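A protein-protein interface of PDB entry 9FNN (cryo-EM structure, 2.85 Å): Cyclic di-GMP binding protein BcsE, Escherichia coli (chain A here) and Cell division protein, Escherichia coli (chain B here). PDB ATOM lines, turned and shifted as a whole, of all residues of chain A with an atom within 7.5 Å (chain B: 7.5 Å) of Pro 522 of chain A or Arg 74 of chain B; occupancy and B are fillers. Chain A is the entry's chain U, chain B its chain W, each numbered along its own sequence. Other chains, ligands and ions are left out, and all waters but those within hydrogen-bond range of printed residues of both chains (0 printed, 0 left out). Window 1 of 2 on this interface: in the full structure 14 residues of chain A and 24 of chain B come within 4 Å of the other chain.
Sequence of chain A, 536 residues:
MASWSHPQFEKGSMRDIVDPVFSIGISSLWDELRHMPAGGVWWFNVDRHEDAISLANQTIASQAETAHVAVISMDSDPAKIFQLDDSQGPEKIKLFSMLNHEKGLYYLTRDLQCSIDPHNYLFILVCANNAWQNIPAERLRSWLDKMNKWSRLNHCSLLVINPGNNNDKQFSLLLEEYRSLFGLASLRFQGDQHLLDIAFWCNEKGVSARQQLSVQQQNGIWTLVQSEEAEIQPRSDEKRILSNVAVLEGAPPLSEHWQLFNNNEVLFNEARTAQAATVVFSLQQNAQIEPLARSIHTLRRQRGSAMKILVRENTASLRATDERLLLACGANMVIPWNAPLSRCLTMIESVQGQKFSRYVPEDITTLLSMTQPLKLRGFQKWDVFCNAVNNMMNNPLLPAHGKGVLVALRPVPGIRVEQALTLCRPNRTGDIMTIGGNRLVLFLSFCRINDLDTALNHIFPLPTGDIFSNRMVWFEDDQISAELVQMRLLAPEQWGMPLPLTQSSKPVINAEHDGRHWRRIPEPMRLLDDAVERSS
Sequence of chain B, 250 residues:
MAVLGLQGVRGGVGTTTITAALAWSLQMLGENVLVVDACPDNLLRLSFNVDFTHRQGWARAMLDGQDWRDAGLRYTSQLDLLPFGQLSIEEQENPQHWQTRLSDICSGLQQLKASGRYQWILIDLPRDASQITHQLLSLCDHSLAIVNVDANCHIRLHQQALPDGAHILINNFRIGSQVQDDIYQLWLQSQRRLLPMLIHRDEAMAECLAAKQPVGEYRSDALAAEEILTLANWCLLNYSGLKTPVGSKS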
ATOM      1  N   ASN A 510     -14.595  18.723 -23.115  1.00  0.00           N
ATOM      2  CA  ASN A 510     -14.071  18.619 -21.755  1.00  0.00           C
ATOM      3  C   ASN A 510     -12.728  17.897 -21.794  1.00  0.00           C
ATOM      4  O   ASN A 510     -12.618  16.694 -21.553  1.00  0.00           O
ATOM      5  CB  ASN A 510     -15.077  17.917 -20.852  1.00  0.00           C
ATOM      6  CG  ASN A 510     -15.520  16.580 -21.397  1.00  0.00           C
ATOM      7  OD1 ASN A 510     -16.301  16.509 -22.341  1.00  0.00           O
ATOM      8  ND2 ASN A 510     -15.026  15.508 -20.797  1.00  0.00           N
ATOM      9  N   ALA A 511     -11.682  18.660 -22.099  1.00  0.00           N
ATOM     10  CA  ALA A 511     -10.335  18.114 -22.148  1.00  0.00           C
ATOM     11  C   ALA A 511      -9.329  19.245 -21.996  1.00  0.00           C
ATOM     12  O   ALA A 511      -9.551  20.348 -22.500  1.00  0.00           O
ATOM     13  CB  ALA A 511     -10.090  17.358 -23.456  1.00  0.00           C
ATOM     14  N   ARG A 519      -5.883  15.243 -20.969  1.00  0.00           N
ATOM     15  CA  ARG A 519      -6.677  14.715 -19.872  1.00  0.00           C
ATOM     16  C   ARG A 519      -8.086  15.272 -19.978  1.00  0.00           C
ATOM     17  O   ARG A 519      -8.268  16.490 -20.077  1.00  0.00           O
ATOM     18  CB  ARG A 519      -6.071  15.075 -18.515  1.00  0.00           C
ATOM     19  CG  ARG A 519      -4.711  14.472 -18.262  1.00  0.00           C
ATOM     20  CD  ARG A 519      -4.287  14.674 -16.823  1.00  0.00           C
ATOM     21  NE  ARG A 519      -2.942  14.171 -16.582  1.00  0.00           N
ATOM     22  CZ  ARG A 519      -2.661  12.928 -16.213  1.00  0.00           C
ATOM     23  NH1 ARG A 519      -3.616  12.031 -16.028  1.00  0.00           N
ATOM     24  NH2 ARG A 519      -1.393  12.577 -16.024  1.00  0.00           N
ATOM     25  N   ARG A 520      -9.074  14.387 -19.958  1.00  0.00           N
ATOM     26  CA  ARG A 520     -10.461  14.814 -20.039  1.00  0.00           C
ATOM     27  C   ARG A 520     -10.988  15.167 -18.657  1.00  0.00           C
ATOM     28  O   ARG A 520     -10.871  14.378 -17.715  1.00  0.00           O
ATOM     29  CB  ARG A 520     -11.320  13.728 -20.674  1.00  0.00           C
ATOM     30  CG  ARG A 520     -11.272  13.739 -22.178  1.00  0.00           C
ATOM     31  CD  ARG A 520     -12.295  12.801 -22.750  1.00  0.00           C
ATOM     32  NE  ARG A 520     -12.502  13.035 -24.170  1.00  0.00           N
ATOM     33  CZ  ARG A 520     -13.497  13.751 -24.670  1.00  0.00           C
ATOM     34  NH1 ARG A 520     -14.396  14.323 -23.887  1.00  0.00           N
ATOM     35  NH2 ARG A 520     -13.596  13.894 -25.988  1.00  0.00           N
ATOM     36  N   ILE A 521     -11.570  16.354 -18.541  1.00  0.00           N
ATOM     37  CA  ILE A 521     -12.085  16.857 -17.273  1.00  0.00           C
ATOM     38  C   ILE A 521     -13.556  16.466 -17.174  1.00  0.00           C
ATOM     39  O   ILE A 521     -14.344  16.855 -18.047  1.00  0.00           O
ATOM     40  CB  ILE A 521     -11.916  18.375 -17.164  1.00  0.00           C
ATOM     41  CG1 ILE A 521     -10.438  18.751 -17.258  1.00  0.00           C
ATOM     42  CG2 ILE A 521     -12.521  18.886 -15.865  1.00  0.00           C
ATOM     43  CD1 ILE A 521     -10.173  20.215 -17.016  1.00  0.00           C
ATOM     44  N   PRO A 522     -13.961  15.707 -16.161  1.00  0.00           N
ATOM     45  CA  PRO A 522     -15.383  15.393 -16.007  1.00  0.00           C
ATOM     46  C   PRO A 522     -16.200  16.653 -15.774  1.00  0.00           C
ATOM     47  O   PRO A 522     -15.757  17.588 -15.106  1.00  0.00           O
ATOM     48  CB  PRO A 522     -15.410  14.465 -14.790  1.00  0.00           C
ATOM     49  CG  PRO A 522     -14.166  14.779 -14.052  1.00  0.00           C
ATOM     50  CD  PRO A 522     -13.148  15.119 -15.087  1.00  0.00           C
ATOM     51  N   GLU A 523     -17.404  16.671 -16.333  1.00  0.00           N
ATOM     52  CA  GLU A 523     -18.290  17.813 -16.218  1.00  0.00           C
ATOM     53  C   GLU A 523     -19.643  17.364 -15.695  1.00  0.00           C
ATOM     54  O   GLU A 523     -20.068  16.235 -15.950  1.00  0.00           O
ATOM     55  CB  GLU A 523     -18.470  18.517 -17.571  1.00  0.00           C
ATOM     56  CG  GLU A 523     -19.126  17.663 -18.632  1.00  0.00           C
ATOM     57  CD  GLU A 523     -19.483  18.455 -19.870  1.00  0.00           C
ATOM     58  OE1 GLU A 523     -19.126  19.649 -19.934  1.00  0.00           O
ATOM     59  OE2 GLU A 523     -20.123  17.886 -20.779  1.00  0.00           O
ATOM     60  N   PRO A 524     -20.334  18.222 -14.950  1.00  0.00           N
ATOM     61  CA  PRO A 524     -21.632  17.829 -14.394  1.00  0.00           C
ATOM     62  C   PRO A 524     -22.675  17.605 -15.476  1.00  0.00           C
ATOM     63  O   PRO A 524     -22.655  18.230 -16.538  1.00  0.00           O
ATOM     64  CB  PRO A 524     -22.007  19.012 -13.497  1.00  0.00           C
ATOM     65  CG  PRO A 524     -21.215  20.155 -14.026  1.00  0.00           C
ATOM     66  CD  PRO A 524     -19.932  19.566 -14.508  1.00  0.00           C
ATOM     67  N   MET A 525     -23.594  16.690 -15.186  1.00  0.00           N
ATOM     68  CA  MET A 525     -24.701  16.379 -16.076  1.00  0.00           C
ATOM     69  C   MET A 525     -25.836  15.817 -15.239  1.00  0.00           C
ATOM     70  O   MET A 525     -25.659  15.466 -14.071  1.00  0.00           O
ATOM     71  CB  MET A 525     -24.293  15.385 -17.165  1.00  0.00           C
ATOM     72  CG  MET A 525     -24.123  13.965 -16.661  1.00  0.00           C
ATOM     73  SD  MET A 525     -23.976  12.754 -17.985  1.00  0.00           S
ATOM     74  CE  MET A 525     -25.558  12.950 -18.799  1.00  0.00           C
ATOM     75  N   ARG A 526     -27.015  15.737 -15.843  1.00  0.00           N
ATOM     76  CA  ARG A 526     -28.189  15.186 -15.182  1.00  0.00           C
ATOM     77  C   ARG A 526     -28.577  13.883 -15.861  1.00  0.00           C
ATOM     78  O   ARG A 526     -28.830  13.860 -17.070  1.00  0.00           O
ATOM     79  CB  ARG A 526     -29.356  16.168 -15.209  1.00  0.00           C
ATOM     80  CG  ARG A 526     -30.530  15.708 -14.372  1.00  0.00           C
ATOM     81  CD  ARG A 526     -31.634  16.740 -14.315  1.00  0.00           C
ATOM     82  NE  ARG A 526     -32.541  16.477 -13.207  1.00  0.00           N
ATOM     83  CZ  ARG A 526     -33.539  15.606 -13.247  1.00  0.00           C
ATOM     84  NH1 ARG A 526     -33.795  14.899 -14.334  1.00  0.00           N
ATOM     85  NH2 ARG A 526     -34.300  15.441 -12.168  1.00  0.00           N
ATOM     86  N   ARG B  45     -14.267   7.536  -8.588  1.00  0.00           N
ATOM     87  CA  ARG B  45     -14.250   8.856  -9.206  1.00  0.00           C
ATOM     88  C   ARG B  45     -12.832   9.330  -9.485  1.00  0.00           C
ATOM     89  O   ARG B  45     -12.596  10.027 -10.476  1.00  0.00           O
ATOM     90  CB  ARG B  45     -14.979   9.857  -8.315  1.00  0.00           C
ATOM     91  CG  ARG B  45     -14.392   9.979  -6.927  1.00  0.00           C
ATOM     92  CD  ARG B  45     -15.154  10.969  -6.084  1.00  0.00           C
ATOM     93  NE  ARG B  45     -14.573  11.094  -4.756  1.00  0.00           N
ATOM     94  CZ  ARG B  45     -13.765  12.076  -4.382  1.00  0.00           C
ATOM     95  NH1 ARG B  45     -13.435  13.051  -5.211  1.00  0.00           N
ATOM     96  NH2 ARG B  45     -13.279  12.079  -3.145  1.00  0.00           N
ATOM     97  N   PHE B  48     -11.316   8.873 -12.857  1.00  0.00           N
ATOM     98  CA  PHE B  48     -11.875   9.662 -13.946  1.00  0.00           C
ATOM     99  C   PHE B  48     -11.638  11.153 -13.735  1.00  0.00           C
ATOM    100  O   PHE B  48     -12.480  11.979 -14.092  1.00  0.00           O
ATOM    101  CB  PHE B  48     -13.364   9.372 -14.114  1.00  0.00           C
ATOM    102  CG  PHE B  48     -13.667   7.936 -14.418  1.00  0.00           C
ATOM    103  CD1 PHE B  48     -13.490   7.433 -15.690  1.00  0.00           C
ATOM    104  CD2 PHE B  48     -14.127   7.089 -13.430  1.00  0.00           C
ATOM    105  CE1 PHE B  48     -13.765   6.116 -15.969  1.00  0.00           C
ATOM    106  CE2 PHE B  48     -14.404   5.771 -13.709  1.00  0.00           C
ATOM    107  CZ  PHE B  48     -14.222   5.286 -14.979  1.00  0.00           C
ATOM    108  N   ASN B  49     -10.495  11.503 -13.144  1.00  0.00           N
ATOM    109  CA  ASN B  49     -10.039  12.888 -13.025  1.00  0.00           C
ATOM    110  C   ASN B  49     -11.017  13.754 -12.238  1.00  0.00           C
ATOM    111  O   ASN B  49     -11.166  14.946 -12.514  1.00  0.00           O
ATOM    112  CB  ASN B  49      -9.776  13.502 -14.402  1.00  0.00           C
ATOM    113  CG  ASN B  49      -8.729  14.588 -14.363  1.00  0.00           C
ATOM    114  OD1 ASN B  49      -8.449  15.159 -13.312  1.00  0.00           O
ATOM    115  ND2 ASN B  49      -8.142  14.879 -15.514  1.00  0.00           N
ATOM    116  N   VAL B  50     -11.687  13.174 -11.254  1.00  0.00           N
ATOM    117  CA  VAL B  50     -12.581  13.920 -10.379  1.00  0.00           C
ATOM    118  C   VAL B  50     -11.781  14.409  -9.183  1.00  0.00           C
ATOM    119  O   VAL B  50     -11.023  13.643  -8.579  1.00  0.00           O
ATOM    120  CB  VAL B  50     -13.772  13.057  -9.934  1.00  0.00           C
ATOM    121  CG1 VAL B  50     -14.694  13.852  -9.043  1.00  0.00           C
ATOM    122  CG2 VAL B  50     -14.525  12.539 -11.138  1.00  0.00           C
ATOM    123  N   ASP B  51     -11.935  15.687  -8.849  1.00  0.00           N
ATOM    124  CA  ASP B  51     -11.194  16.260  -7.737  1.00  0.00           C
ATOM    125  C   ASP B  51     -11.584  15.588  -6.427  1.00  0.00           C
ATOM    126  O   ASP B  51     -12.732  15.189  -6.222  1.00  0.00           O
ATOM    127  CB  ASP B  51     -11.445  17.764  -7.646  1.00  0.00           C
ATOM    128  CG  ASP B  51     -10.844  18.523  -8.806  1.00  0.00           C
ATOM    129  OD1 ASP B  51      -9.821  18.063  -9.354  1.00  0.00           O
ATOM    130  OD2 ASP B  51     -11.393  19.584  -9.170  1.00  0.00           O
ATOM    131  N   ALA B  71     -26.173  14.306  -9.685  1.00  0.00           N
ATOM    132  CA  ALA B  71     -24.849  13.940  -9.205  1.00  0.00           C
ATOM    133  C   ALA B  71     -24.033  13.190 -10.245  1.00  0.00           C
ATOM    134  O   ALA B  71     -22.987  12.631  -9.908  1.00  0.00           O
ATOM    135  CB  ALA B  71     -24.966  13.102  -7.934  1.00  0.00           C
ATOM    136  N   GLY B  72     -24.489  13.154 -11.492  1.00  0.00           N
ATOM    137  CA  GLY B  72     -23.787  12.437 -12.533  1.00  0.00           C
ATOM    138  C   GLY B  72     -22.749  13.292 -13.232  1.00  0.00           C
ATOM    139  O   GLY B  72     -22.911  14.498 -13.391  1.00  0.00           O
ATOM    140  N   LEU B  73     -21.667  12.644 -13.652  1.00  0.00           N
ATOM    141  CA  LEU B  73     -20.572  13.304 -14.343  1.00  0.00           C
ATOM    142  C   LEU B  73     -20.358  12.661 -15.703  1.00  0.00           C
ATOM    143  O   LEU B  73     -20.401  11.436 -15.837  1.00  0.00           O
ATOM    144  CB  LEU B  73     -19.282  13.233 -13.529  1.00  0.00           C
ATOM    145  CG  LEU B  73     -19.267  13.975 -12.197  1.00  0.00           C
ATOM    146  CD1 LEU B  73     -17.955  13.742 -11.485  1.00  0.00           C
ATOM    147  CD2 LEU B  73     -19.495  15.455 -12.413  1.00  0.00           C
ATOM    148  N   ARG B  74     -20.125  13.495 -16.708  1.00  0.00           N
ATOM    149  CA  ARG B  74     -19.860  13.045 -18.065  1.00  0.00           C
ATOM    150  C   ARG B  74     -18.359  13.075 -18.310  1.00  0.00           C
ATOM    151  O   ARG B  74     -17.729  14.129 -18.187  1.00  0.00           O
ATOM    152  CB  ARG B  74     -20.582  13.928 -19.079  1.00  0.00           C
ATOM    153  CG  ARG B  74     -20.254  13.607 -20.523  1.00  0.00           C
ATOM    154  CD  ARG B  74     -20.818  14.655 -21.462  1.00  0.00           C
ATOM    155  NE  ARG B  74     -22.256  14.814 -21.299  1.00  0.00           N
ATOM    156  CZ  ARG B  74     -23.166  14.085 -21.930  1.00  0.00           C
ATOM    157  NH1 ARG B  74     -22.819  13.128 -22.775  1.00  0.00           N
ATOM    158  NH2 ARG B  74     -24.456  14.322 -21.707  1.00  0.00           N
ATOM    159  N   TYR B  75     -17.789  11.922 -18.654  1.00  0.00           N
ATOM    160  CA  TYR B  75     -16.369  11.845 -18.977  1.00  0.00           C
ATOM    161  C   TYR B  75     -16.147  11.981 -20.481  1.00  0.00           C
ATOM    162  O   TYR B  75     -15.412  12.866 -20.932  1.00  0.00           O
ATOM    163  CB  TYR B  75     -15.783  10.533 -18.447  1.00  0.00           C
ATOM    164  CG  TYR B  75     -14.277  10.520 -18.377  1.00  0.00           C
ATOM    165  CD1 TYR B  75     -13.601  11.341 -17.493  1.00  0.00           C
ATOM    166  CD2 TYR B  75     -13.534   9.683 -19.189  1.00  0.00           C
ATOM    167  CE1 TYR B  75     -12.230  11.335 -17.424  1.00  0.00           C
ATOM    168  CE2 TYR B  75     -12.161   9.669 -19.126  1.00  0.00           C
ATOM    169  CZ  TYR B  75     -11.515  10.496 -18.240  1.00  0.00           C
ATOM    170  OH  TYR B  75     -10.143  10.488 -18.172  1.00  0.00           O
ATOM    171  N   THR B  76     -16.777  11.112 -21.265  1.00  0.00           N
ATOM    172  CA  THR B  76     -16.801  11.204 -22.717  1.00  0.00           C
ATOM    173  C   THR B  76     -18.255  11.180 -23.172  1.00  0.00           C
ATOM    174  O   THR B  76     -19.181  11.118 -22.360  1.00  0.00           O
ATOM    175  CB  THR B  76     -16.011  10.066 -23.372  1.00  0.00           C
ATOM    176  OG1 THR B  76     -16.691   8.823 -23.158  1.00  0.00           O
ATOM    177  CG2 THR B  76     -14.621   9.976 -22.784  1.00  0.00           C
ATOM    178  N   SER B  77     -18.458  11.228 -24.488  1.00  0.00           N
ATOM    179  CA  SER B  77     -19.812  11.188 -25.023  1.00  0.00           C
ATOM    180  C   SER B  77     -20.483   9.841 -24.795  1.00  0.00           C
ATOM    181  O   SER B  77     -21.714   9.762 -24.842  1.00  0.00           O
ATOM    182  CB  SER B  77     -19.801  11.514 -26.515  1.00  0.00           C
ATOM    183  OG  SER B  77     -19.187  10.478 -27.256  1.00  0.00           O
ATOM    184  N   GLN B  78     -19.705   8.786 -24.550  1.00  0.00           N
ATOM    185  CA  GLN B  78     -20.238   7.443 -24.360  1.00  0.00           C
ATOM    186  C   GLN B  78     -19.831   6.843 -23.020  1.00  0.00           C
ATOM    187  O   GLN B  78     -19.832   5.618 -22.870  1.00  0.00           O
ATOM    188  CB  GLN B  78     -19.794   6.532 -25.504  1.00  0.00           C
ATOM    189  CG  GLN B  78     -20.287   6.978 -26.868  1.00  0.00           C
ATOM    190  CD  GLN B  78     -19.696   6.162 -27.995  1.00  0.00           C
ATOM    191  OE1 GLN B  78     -18.481   5.994 -28.084  1.00  0.00           O
ATOM    192  NE2 GLN B  78     -20.554   5.646 -28.864  1.00  0.00           N
ATOM    193  N   LEU B  79     -19.479   7.674 -22.044  1.00  0.00           N
ATOM    194  CA  LEU B  79     -19.114   7.183 -20.718  1.00  0.00           C
ATOM    195  C   LEU B  79     -19.590   8.182 -19.678  1.00  0.00           C
ATOM    196  O   LEU B  79     -19.185   9.347 -19.706  1.00  0.00           O
ATOM    197  CB  LEU B  79     -17.605   6.962 -20.607  1.00  0.00           C
ATOM    198  CG  LEU B  79     -17.092   6.388 -19.287  1.00  0.00           C
ATOM    199  CD1 LEU B  79     -17.875   5.154 -18.899  1.00  0.00           C
ATOM    200  CD2 LEU B  79     -15.620   6.066 -19.393  1.00  0.00           C
ATOM    201  N   ASP B  80     -20.444   7.726 -18.767  1.00  0.00           N
ATOM    202  CA  ASP B  80     -20.971   8.546 -17.689  1.00  0.00           C
ATOM    203  C   ASP B  80     -20.630   7.912 -16.351  1.00  0.00           C
ATOM    204  O   ASP B  80     -20.546   6.688 -16.229  1.00  0.00           O
ATOM    205  CB  ASP B  80     -22.485   8.724 -17.810  1.00  0.00           C
ATOM    206  CG  ASP B  80     -22.875   9.591 -18.987  1.00  0.00           C
ATOM    207  OD1 ASP B  80     -21.969  10.149 -19.640  1.00  0.00           O
ATOM    208  OD2 ASP B  80     -24.087   9.715 -19.261  1.00  0.00           O
ATOM    209  N   LEU B  81     -20.436   8.758 -15.347  1.00  0.00           N
ATOM    210  CA  LEU B  81     -19.972   8.340 -14.036  1.00  0.00           C
ATOM    211  C   LEU B  81     -20.921   8.855 -12.967  1.00  0.00           C
ATOM    212  O   LEU B  81     -21.331  10.019 -12.998  1.00  0.00           O
ATOM    213  CB  LEU B  81     -18.551   8.856 -13.782  1.00  0.00           C
ATOM    214  CG  LEU B  81     -18.049   8.939 -12.343  1.00  0.00           C
ATOM    215  CD1 LEU B  81     -17.940   7.562 -11.717  1.00  0.00           C
ATOM    216  CD2 LEU B  81     -16.716   9.650 -12.300  1.00  0.00           C
ATOM    217  N   LEU B  82     -21.268   7.985 -12.020  1.00  0.00           N
ATOM    218  CA  LEU B  82     -22.136   8.333 -10.897  1.00  0.00           C
ATOM    219  C   LEU B  82     -21.398   8.018  -9.605  1.00  0.00           C
ATOM    220  O   LEU B  82     -21.450   6.887  -9.106  1.00  0.00           O
ATOM    221  CB  LEU B  82     -23.467   7.591 -10.970  1.00  0.00           C
ATOM    222  CG  LEU B  82     -24.550   8.063 -10.001  1.00  0.00           C
ATOM    223  CD1 LEU B  82     -24.908   9.508 -10.274  1.00  0.00           C
ATOM    224  CD2 LEU B  82     -25.777   7.183 -10.095  1.00  0.00           C
ATOM    225  N   ARG B 117     -30.968   4.394 -22.861  1.00  0.00           N
ATOM    226  CA  ARG B 117     -29.873   5.314 -23.147  1.00  0.00           C
ATOM    227  C   ARG B 117     -28.517   4.654 -22.953  1.00  0.00           C
ATOM    228  O   ARG B 117     -27.558   4.992 -23.655  1.00  0.00           O
ATOM    229  CB  ARG B 117     -29.982   6.552 -22.261  1.00  0.00           C
ATOM    230  CG  ARG B 117     -30.519   7.780 -22.970  1.00  0.00           C
ATOM    231  CD  ARG B 117     -29.471   8.399 -23.882  1.00  0.00           C
ATOM    232  NE  ARG B 117     -28.408   9.058 -23.130  1.00  0.00           N
ATOM    233  CZ  ARG B 117     -27.225   8.518 -22.869  1.00  0.00           C
ATOM    234  NH1 ARG B 117     -26.910   7.305 -23.289  1.00  0.00           N
ATOM    235  NH2 ARG B 117     -26.335   9.216 -22.169  1.00  0.00           N
ATOM    236  N   TYR B 118     -28.417   3.720 -22.013  1.00  0.00           N
ATOM    237  CA  TYR B 118     -27.159   3.082 -21.658  1.00  0.00           C
ATOM    238  C   TYR B 118     -27.205   1.608 -22.029  1.00  0.00           C
ATOM    239  O   TYR B 118     -28.132   0.892 -21.635  1.00  0.00           O
ATOM    240  CB  TYR B 118     -26.874   3.243 -20.164  1.00  0.00           C
ATOM    241  CG  TYR B 118     -26.626   4.670 -19.744  1.00  0.00           C
ATOM    242  CD1 TYR B 118     -25.674   5.446 -20.384  1.00  0.00           C
ATOM    243  CD2 TYR B 118     -27.351   5.245 -18.713  1.00  0.00           C
ATOM    244  CE1 TYR B 118     -25.444   6.748 -20.004  1.00  0.00           C
ATOM    245  CE2 TYR B 118     -27.128   6.548 -18.329  1.00  0.00           C
ATOM    246  CZ  TYR B 118     -26.175   7.294 -18.977  1.00  0.00           C
ATOM    247  OH  TYR B 118     -25.951   8.595 -18.596  1.00  0.00           O
ATOM    248  N   LYS B 212      -4.726   9.419 -12.410  1.00  0.00           N
ATOM    249  CA  LYS B 212      -6.152   9.738 -12.446  1.00  0.00           C
ATOM    250  C   LYS B 212      -6.734   9.535 -13.845  1.00  0.00           C
ATOM    251  O   LYS B 212      -7.454  10.382 -14.376  1.00  0.00           O
ATOM    252  CB  LYS B 212      -6.407  11.157 -11.936  1.00  0.00           C
ATOM    253  CG  LYS B 212      -5.752  11.442 -10.595  1.00  0.00           C
ATOM    254  CD  LYS B 212      -6.161  12.791 -10.042  1.00  0.00           C
ATOM    255  CE  LYS B 212      -7.554  12.744  -9.461  1.00  0.00           C
ATOM    256  NZ  LYS B 212      -7.979  14.075  -8.965  1.00  0.00           N
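The backbone carbonyl oxygen (O) of Tyr 75 of chain B sits at hydrogen-bond distance from the guanidinium group (NH1) of Arg 520 of chain A (3.4 Å). The side-chain sulfur (SD) of Met 525 of chain A sits close to the side-chain carboxylate (OD2) of Asp 80 of chain B (3.3 Å). N of Met 525 of chain A lies within hydrogen-bond range of O of Gly 72 of chain B. OE2 of Glu 523 of chain A is in salt-bridge range of NE of Arg 74 of chain B (3.8 Å). The side-chain amide nitrogen of Asn 510 of chain A sits at hydrogen-bond distance from the backbone carbonyl oxygen of Tyr 75 of chain B.
The side-chain hydroxyl of Thr 76 of chain B sits close to the backbone NH of Gln 78 of chain B (3.3 Å). O of Leu 73 of chain B sits at hydrogen-bond distance from N of Leu 81 of chain B, 2.7 Å away. The guanidinium group of Arg 117 of chain B is in salt-bridge range of the side-chain carboxylate of Asp 80 of chain B. The backbone carbonyl oxygen (O) of Lys 212 of chain B lies within hydrogen-bond range of the backbone NH (N) of Asn 49 of chain B. The backbone NH (N) of Val 50 of chain B sits close to the backbone carbonyl oxygen (O) of Arg 45 of chain B (3.4 Å). The side-chain amide nitrogen of Asn 510 of chain A lies close to the backbone carbonyl oxygen of Ile 521 of chain A (3.1 Å).
Asn 49 of chain B touches Arg 519 of chain A. Asn 49 of chain B touches Arg 520 of chain A (ND2 to O, 3.5 Å). Thr 76 of chain B touches Arg 520 of chain A (CG2 to CD, 3.7 Å). Phe 48 of chain B touches Pro 522 of chain A. Pro 522 of chain A touches Asn 49 of chain B (CD to O, 3.3 Å). CG2 of Val 50 of chain B touches CG of Pro 522 of chain A, at 3.7 Å. CA of Pro 522 of chain A touches O of Arg 74 of chain B, 3.4 Å away. O of Gly 72 of chain B touches CA of Pro 524 of chain A (3.7 Å). CA of Pro 524 of chain A touches CD2 of Leu 73 of chain B, 3.8 Å away. Met 525 of chain A touches Arg 74 of chain B.
Pro 522 of chain A touches just these residues of chain B: Phe 48, Asn 49, Val 50 and Arg 74. Of the printed residues of chain A, Arg 74 of chain B touches Pro 522 (3.4 Å), Glu 523 (2.8 Å) and Met 525 (3.4 Å). Printed residues of chain A within 4 Å of Leu 73 of chain B: Glu 523 and Pro 524. Of the printed residues of chain A, Asp 80 of chain B touches Met 525. The nearest residue of chain B that does not touch Pro 522 of chain A is Leu 73 of chain B (4.2 Å). The nearest printed residue of chain A that does not touch Tyr 75 of chain B is Pro 522 of chain A (4.5 Å).
Of the 10 printed residues of chain A, 7 touch a printed residue of chain B. Among the printed residues, 16 pairs touch across the chains.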
